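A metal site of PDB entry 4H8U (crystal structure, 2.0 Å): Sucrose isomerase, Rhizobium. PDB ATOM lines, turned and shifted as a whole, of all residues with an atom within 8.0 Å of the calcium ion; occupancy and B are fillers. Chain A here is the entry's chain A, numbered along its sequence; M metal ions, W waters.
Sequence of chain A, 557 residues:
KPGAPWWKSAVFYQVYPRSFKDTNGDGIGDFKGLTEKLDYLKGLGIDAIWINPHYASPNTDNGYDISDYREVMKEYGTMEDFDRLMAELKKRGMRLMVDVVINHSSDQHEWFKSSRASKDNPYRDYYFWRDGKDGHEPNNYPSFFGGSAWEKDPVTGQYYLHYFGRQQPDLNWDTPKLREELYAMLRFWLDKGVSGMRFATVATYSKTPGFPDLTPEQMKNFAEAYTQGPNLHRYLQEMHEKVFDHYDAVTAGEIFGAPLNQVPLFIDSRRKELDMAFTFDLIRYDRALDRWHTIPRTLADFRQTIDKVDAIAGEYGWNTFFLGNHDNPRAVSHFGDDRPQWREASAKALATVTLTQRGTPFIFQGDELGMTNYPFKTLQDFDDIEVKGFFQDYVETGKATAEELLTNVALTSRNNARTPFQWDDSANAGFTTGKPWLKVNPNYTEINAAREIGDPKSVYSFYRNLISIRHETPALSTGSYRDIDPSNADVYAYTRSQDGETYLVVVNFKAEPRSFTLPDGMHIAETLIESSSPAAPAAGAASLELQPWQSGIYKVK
OD1 of Asp 30 is in hydrogen-bond range of OG1 of Thr 23 (2.6 Å).
The backbone carbonyl oxygen (O) of Lys 21 lies within hydrogen-bond range of the backbone NH (N) of Asp 30 (3.1 Å).
The side-chain carboxylate of Asp 30 sits at hydrogen-bond distance from the backbone NH of Gly 33 (2.9 Å).
N of Gly 25 lies within hydrogen-bond range of OD2 of Asp 22, 3.2 Å away.
N of Gly 27 is in hydrogen-bond range of OD2 of Asp 22, at 2.7 Å.
OD2 of Asp 22 is in hydrogen-bond range of OG1 of Thr 432.
The backbone NH (N) of Asp 22 lies within hydrogen-bond range of the backbone carbonyl oxygen (O) of Phe 431 (3.0 Å).
Of the 21 residues printed, 5 come within 4 Å of the calcium ion.
The calcium ion is bound by water W1, OD1 of Asn 24, OD2 of Asp 30, OD1 of Asp 22, OD1 of Asp 26, O of Ile 28 and water W2.
The calcium ion has seven donor atoms within binding distance.
Water W2 lies within hydrogen-bond range of the side-chain amide nitrogen of Asn 24 and the backbone carbonyl oxygen of Glu 75.
Water W1 bridges the side-chain carboxylate (OD2) of Asp 26 (2.7 Å) and the backbone carbonyl oxygen (O) of Glu 75 (2.7 Å).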
ATOM      1  N   PRO A  17      -0.996 -27.757  23.240  1.00  0.00           N
ATOM      2  CA  PRO A  17      -1.084 -26.878  22.061  1.00  0.00           C
ATOM      3  C   PRO A  17      -2.179 -27.223  21.049  1.00  0.00           C
ATOM      4  O   PRO A  17      -2.713 -26.317  20.374  1.00  0.00           O
ATOM      5  CB  PRO A  17       0.321 -26.974  21.416  1.00  0.00           C
ATOM      6  CG  PRO A  17       1.216 -27.341  22.544  1.00  0.00           C
ATOM      7  CD  PRO A  17       0.375 -28.266  23.445  1.00  0.00           C
ATOM      8  N   ARG A  18      -2.480 -28.500  20.899  1.00  0.00           N
ATOM      9  CA  ARG A  18      -3.489 -28.923  19.935  1.00  0.00           C
ATOM     10  C   ARG A  18      -4.828 -28.180  20.167  1.00  0.00           C
ATOM     11  O   ARG A  18      -5.624 -28.004  19.234  1.00  0.00           O
ATOM     12  CB  ARG A  18      -3.677 -30.435  20.026  1.00  0.00           C
ATOM     13  CG  ARG A  18      -4.536 -31.079  18.950  1.00  0.00           C
ATOM     14  CD  ARG A  18      -4.706 -32.592  19.203  1.00  0.00           C
ATOM     15  NE  ARG A  18      -5.565 -33.171  18.173  1.00  0.00           N
ATOM     16  CZ  ARG A  18      -5.131 -33.589  16.984  1.00  0.00           C
ATOM     17  NH1 ARG A  18      -3.832 -33.533  16.701  1.00  0.00           N
ATOM     18  NH2 ARG A  18      -5.978 -34.101  16.085  1.00  0.00           N
ATOM     19  N   LYS A  21      -4.814 -22.528  20.541  1.00  0.00           N
ATOM     20  CA  LYS A  21      -5.176 -21.475  19.603  1.00  0.00           C
ATOM     21  C   LYS A  21      -4.685 -21.838  18.227  1.00  0.00           C
ATOM     22  O   LYS A  21      -3.482 -21.994  18.029  1.00  0.00           O
ATOM     23  CB  LYS A  21      -4.573 -20.119  20.027  1.00  0.00           C
ATOM     24  CG  LYS A  21      -4.950 -18.931  19.132  1.00  0.00           C
ATOM     25  CD  LYS A  21      -6.392 -18.454  19.324  1.00  0.00           C
ATOM     26  CE  LYS A  21      -6.900 -17.669  18.096  1.00  0.00           C
ATOM     27  NZ  LYS A  21      -5.936 -16.735  17.449  1.00  0.00           N
ATOM     28  N   ASP A  22      -5.628 -21.988  17.298  1.00  0.00           N
ATOM     29  CA  ASP A  22      -5.334 -22.261  15.896  1.00  0.00           C
ATOM     30  C   ASP A  22      -5.072 -20.925  15.167  1.00  0.00           C
ATOM     31  O   ASP A  22      -5.776 -19.931  15.412  1.00  0.00           O
ATOM     32  CB  ASP A  22      -6.544 -22.999  15.260  1.00  0.00           C
ATOM     33  CG  ASP A  22      -6.349 -23.312  13.757  1.00  0.00           C
ATOM     34  OD1 ASP A  22      -5.233 -23.138  13.244  1.00  0.00           O
ATOM     35  OD2 ASP A  22      -7.292 -23.823  13.126  1.00  0.00           O
ATOM     36  N   THR A  23      -4.090 -20.887  14.266  1.00  0.00           N
ATOM     37  CA  THR A  23      -3.851 -19.658  13.509  1.00  0.00           C
ATOM     38  C   THR A  23      -3.976 -19.849  12.007  1.00  0.00           C
ATOM     39  O   THR A  23      -3.708 -18.898  11.267  1.00  0.00           O
ATOM     40  CB  THR A  23      -2.476 -19.004  13.809  1.00  0.00           C
ATOM     41  OG1 THR A  23      -1.442 -19.965  13.590  1.00  0.00           O
ATOM     42  CG2 THR A  23      -2.405 -18.532  15.249  1.00  0.00           C
ATOM     43  N   ASN A  24      -4.351 -21.046  11.552  1.00  0.00           N
ATOM     44  CA  ASN A  24      -4.512 -21.264  10.108  1.00  0.00           C
ATOM     45  C   ASN A  24      -5.792 -21.979   9.641  1.00  0.00           C
ATOM     46  O   ASN A  24      -5.821 -22.521   8.534  1.00  0.00           O
ATOM     47  CB  ASN A  24      -3.291 -22.007   9.527  1.00  0.00           C
ATOM     48  CG  ASN A  24      -3.238 -23.450   9.948  1.00  0.00           C
ATOM     49  OD1 ASN A  24      -3.792 -23.806  10.994  1.00  0.00           O
ATOM     50  ND2 ASN A  24      -2.593 -24.300   9.151  1.00  0.00           N
ATOM     51  N   GLY A  25      -6.818 -22.038  10.478  1.00  0.00           N
ATOM     52  CA  GLY A  25      -8.108 -22.626  10.064  1.00  0.00           C
ATOM     53  C   GLY A  25      -8.237 -24.152   9.989  1.00  0.00           C
ATOM     54  O   GLY A  25      -9.338 -24.684   9.742  1.00  0.00           O
ATOM     55  N   ASP A  26      -7.135 -24.866  10.209  1.00  0.00           N
ATOM     56  CA  ASP A  26      -7.194 -26.316  10.119  1.00  0.00           C
ATOM     57  C   ASP A  26      -7.890 -26.950  11.330  1.00  0.00           C
ATOM     58  O   ASP A  26      -8.026 -28.148  11.389  1.00  0.00           O
ATOM     59  CB  ASP A  26      -5.819 -26.928   9.858  1.00  0.00           C
ATOM     60  CG  ASP A  26      -4.888 -26.895  11.098  1.00  0.00           C
ATOM     61  OD1 ASP A  26      -5.207 -26.300  12.152  1.00  0.00           O
ATOM     62  OD2 ASP A  26      -3.814 -27.507  10.995  1.00  0.00           O
ATOM     63  N   GLY A  27      -8.344 -26.127  12.271  1.00  0.00           N
ATOM     64  CA  GLY A  27      -9.010 -26.660  13.461  1.00  0.00           C
ATOM     65  C   GLY A  27      -8.067 -27.233  14.517  1.00  0.00           C
ATOM     66  O   GLY A  27      -8.524 -27.787  15.521  1.00  0.00           O
ATOM     67  N   ILE A  28      -6.761 -27.076  14.318  1.00  0.00           N
ATOM     68  CA  ILE A  28      -5.785 -27.590  15.336  1.00  0.00           C
ATOM     69  C   ILE A  28      -4.969 -26.422  15.894  1.00  0.00           C
ATOM     70  O   ILE A  28      -4.521 -25.576  15.145  1.00  0.00           O
ATOM     71  CB  ILE A  28      -4.892 -28.734  14.775  1.00  0.00           C
ATOM     72  CG1 ILE A  28      -5.759 -29.960  14.459  1.00  0.00           C
ATOM     73  CG2 ILE A  28      -3.759 -29.099  15.733  1.00  0.00           C
ATOM     74  CD1 ILE A  28      -5.239 -30.829  13.320  1.00  0.00           C
ATOM     75  N   GLY A  29      -4.814 -26.319  17.212  1.00  0.00           N
ATOM     76  CA  GLY A  29      -3.940 -25.260  17.745  1.00  0.00           C
ATOM     77  C   GLY A  29      -2.491 -25.479  17.325  1.00  0.00           C
ATOM     78  O   GLY A  29      -2.084 -26.587  17.026  1.00  0.00           O
ATOM     79  N   ASP A  30      -1.700 -24.418  17.319  1.00  0.00           N
ATOM     80  CA  ASP A  30      -0.372 -24.483  16.744  1.00  0.00           C
ATOM     81  C   ASP A  30       0.553 -23.516  17.494  1.00  0.00           C
ATOM     82  O   ASP A  30       0.085 -22.776  18.341  1.00  0.00           O
ATOM     83  CB  ASP A  30      -0.396 -24.129  15.250  1.00  0.00           C
ATOM     84  CG  ASP A  30      -1.282 -22.929  14.953  1.00  0.00           C
ATOM     85  OD1 ASP A  30      -0.961 -21.802  15.367  1.00  0.00           O
ATOM     86  OD2 ASP A  30      -2.351 -23.138  14.317  1.00  0.00           O
ATOM     87  N   PHE A  31       1.837 -23.530  17.139  1.00  0.00           N
ATOM     88  CA  PHE A  31       2.849 -22.716  17.811  1.00  0.00           C
ATOM     89  C   PHE A  31       2.548 -21.238  17.629  1.00  0.00           C
ATOM     90  O   PHE A  31       2.527 -20.472  18.613  1.00  0.00           O
ATOM     91  CB  PHE A  31       4.261 -23.050  17.292  1.00  0.00           C
ATOM     92  CG  PHE A  31       4.827 -24.377  17.789  1.00  0.00           C
ATOM     93  CD1 PHE A  31       4.723 -24.761  19.127  1.00  0.00           C
ATOM     94  CD2 PHE A  31       5.556 -25.187  16.919  1.00  0.00           C
ATOM     95  CE1 PHE A  31       5.289 -25.953  19.569  1.00  0.00           C
ATOM     96  CE2 PHE A  31       6.104 -26.383  17.347  1.00  0.00           C
ATOM     97  CZ  PHE A  31       5.973 -26.770  18.677  1.00  0.00           C
ATOM     98  N   LYS A  32       2.313 -20.804  16.381  1.00  0.00           N
ATOM     99  CA  LYS A  32       1.990 -19.391  16.176  1.00  0.00           C
ATOM    100  C   LYS A  32       0.858 -18.935  17.099  1.00  0.00           C
ATOM    101  O   LYS A  32       0.898 -17.830  17.642  1.00  0.00           O
ATOM    102  CB  LYS A  32       1.617 -19.084  14.725  1.00  0.00           C
ATOM    103  CG  LYS A  32       2.771 -19.339  13.770  1.00  0.00           C
ATOM    104  N   GLY A  33      -0.127 -19.820  17.304  1.00  0.00           N
ATOM    105  CA  GLY A  33      -1.260 -19.435  18.136  1.00  0.00           C
ATOM    106  C   GLY A  33      -0.856 -19.275  19.587  1.00  0.00           C
ATOM    107  O   GLY A  33      -1.350 -18.382  20.286  1.00  0.00           O
ATOM    108  N   LYS A  74       4.258 -31.469  12.539  1.00  0.00           N
ATOM    109  CA  LYS A  74       3.808 -30.724  11.354  1.00  0.00           C
ATOM    110  C   LYS A  74       2.564 -29.855  11.642  1.00  0.00           C
ATOM    111  O   LYS A  74       2.468 -28.700  11.210  1.00  0.00           O
ATOM    112  CB  LYS A  74       3.540 -31.679  10.177  1.00  0.00           C
ATOM    113  N   GLU A  75       1.616 -30.380  12.409  1.00  0.00           N
ATOM    114  CA  GLU A  75       0.464 -29.561  12.804  1.00  0.00           C
ATOM    115  C   GLU A  75       0.840 -28.305  13.603  1.00  0.00           C
ATOM    116  O   GLU A  75       0.137 -27.287  13.513  1.00  0.00           O
ATOM    117  CB  GLU A  75      -0.559 -30.380  13.624  1.00  0.00           C
ATOM    118  CG  GLU A  75      -1.400 -31.384  12.836  1.00  0.00           C
ATOM    119  CD  GLU A  75      -0.658 -32.655  12.432  1.00  0.00           C
ATOM    120  OE1 GLU A  75       0.454 -32.930  12.952  1.00  0.00           O
ATOM    121  OE2 GLU A  75      -1.230 -33.416  11.611  1.00  0.00           O
ATOM    122  N   TYR A  76       1.901 -28.358  14.423  1.00  0.00           N
ATOM    123  CA  TYR A  76       2.191 -27.159  15.230  1.00  0.00           C
ATOM    124  C   TYR A  76       2.985 -26.060  14.486  1.00  0.00           C
ATOM    125  O   TYR A  76       2.922 -24.909  14.882  1.00  0.00           O
ATOM    126  CB  TYR A  76       2.761 -27.463  16.646  1.00  0.00           C
ATOM    127  CG  TYR A  76       1.913 -28.438  17.466  1.00  0.00           C
ATOM    128  CD1 TYR A  76       0.567 -28.655  17.160  1.00  0.00           C
ATOM    129  CD2 TYR A  76       2.464 -29.145  18.546  1.00  0.00           C
ATOM    130  CE1 TYR A  76      -0.204 -29.562  17.895  1.00  0.00           C
ATOM    131  CE2 TYR A  76       1.696 -30.028  19.309  1.00  0.00           C
ATOM    132  CZ  TYR A  76       0.371 -30.236  18.979  1.00  0.00           C
ATOM    133  OH  TYR A  76      -0.400 -31.145  19.692  1.00  0.00           O
ATOM    134  N   GLY A  77       3.701 -26.427  13.426  1.00  0.00           N
ATOM    135  CA  GLY A  77       4.526 -25.478  12.667  1.00  0.00           C
ATOM    136  C   GLY A  77       5.847 -26.083  12.239  1.00  0.00           C
ATOM    137  O   GLY A  77       5.886 -27.252  11.882  1.00  0.00           O
ATOM    138  N   PHE A 431     -11.338 -19.796  18.939  1.00  0.00           N
ATOM    139  CA  PHE A 431     -10.275 -20.780  18.856  1.00  0.00           C
ATOM    140  C   PHE A 431      -9.737 -20.973  17.428  1.00  0.00           C
ATOM    141  O   PHE A 431      -8.527 -21.108  17.223  1.00  0.00           O
ATOM    142  CB  PHE A 431     -10.705 -22.137  19.438  1.00  0.00           C
ATOM    143  CG  PHE A 431      -9.776 -23.264  19.096  1.00  0.00           C
ATOM    144  CD1 PHE A 431      -8.543 -23.392  19.745  1.00  0.00           C
ATOM    145  CD2 PHE A 431     -10.114 -24.184  18.109  1.00  0.00           C
ATOM    146  CE1 PHE A 431      -7.685 -24.423  19.402  1.00  0.00           C
ATOM    147  CE2 PHE A 431      -9.264 -25.226  17.772  1.00  0.00           C
ATOM    148  CZ  PHE A 431      -8.050 -25.344  18.429  1.00  0.00           C
ATOM    149  N   THR A 432     -10.643 -20.994  16.447  1.00  0.00           N
ATOM    150  CA  THR A 432     -10.286 -21.270  15.059  1.00  0.00           C
ATOM    151  C   THR A 432     -11.285 -20.566  14.137  1.00  0.00           C
ATOM    152  O   THR A 432     -12.424 -20.312  14.525  1.00  0.00           O
ATOM    153  CB  THR A 432     -10.320 -22.775  14.737  1.00  0.00           C
ATOM    154  OG1 THR A 432      -9.784 -23.015  13.431  1.00  0.00           O
ATOM    155  CG2 THR A 432     -11.750 -23.352  14.806  1.00  0.00           C
HETATM  156 CA    CA M   1      -3.507 -24.763  13.030  1.00  0.00          CA
HETATM  157  O   HOH W   1      -2.547 -26.771  13.269  1.00  0.00           O
HETATM  158  O   HOH W   2      -1.165 -24.488  12.059  1.00  0.00           O
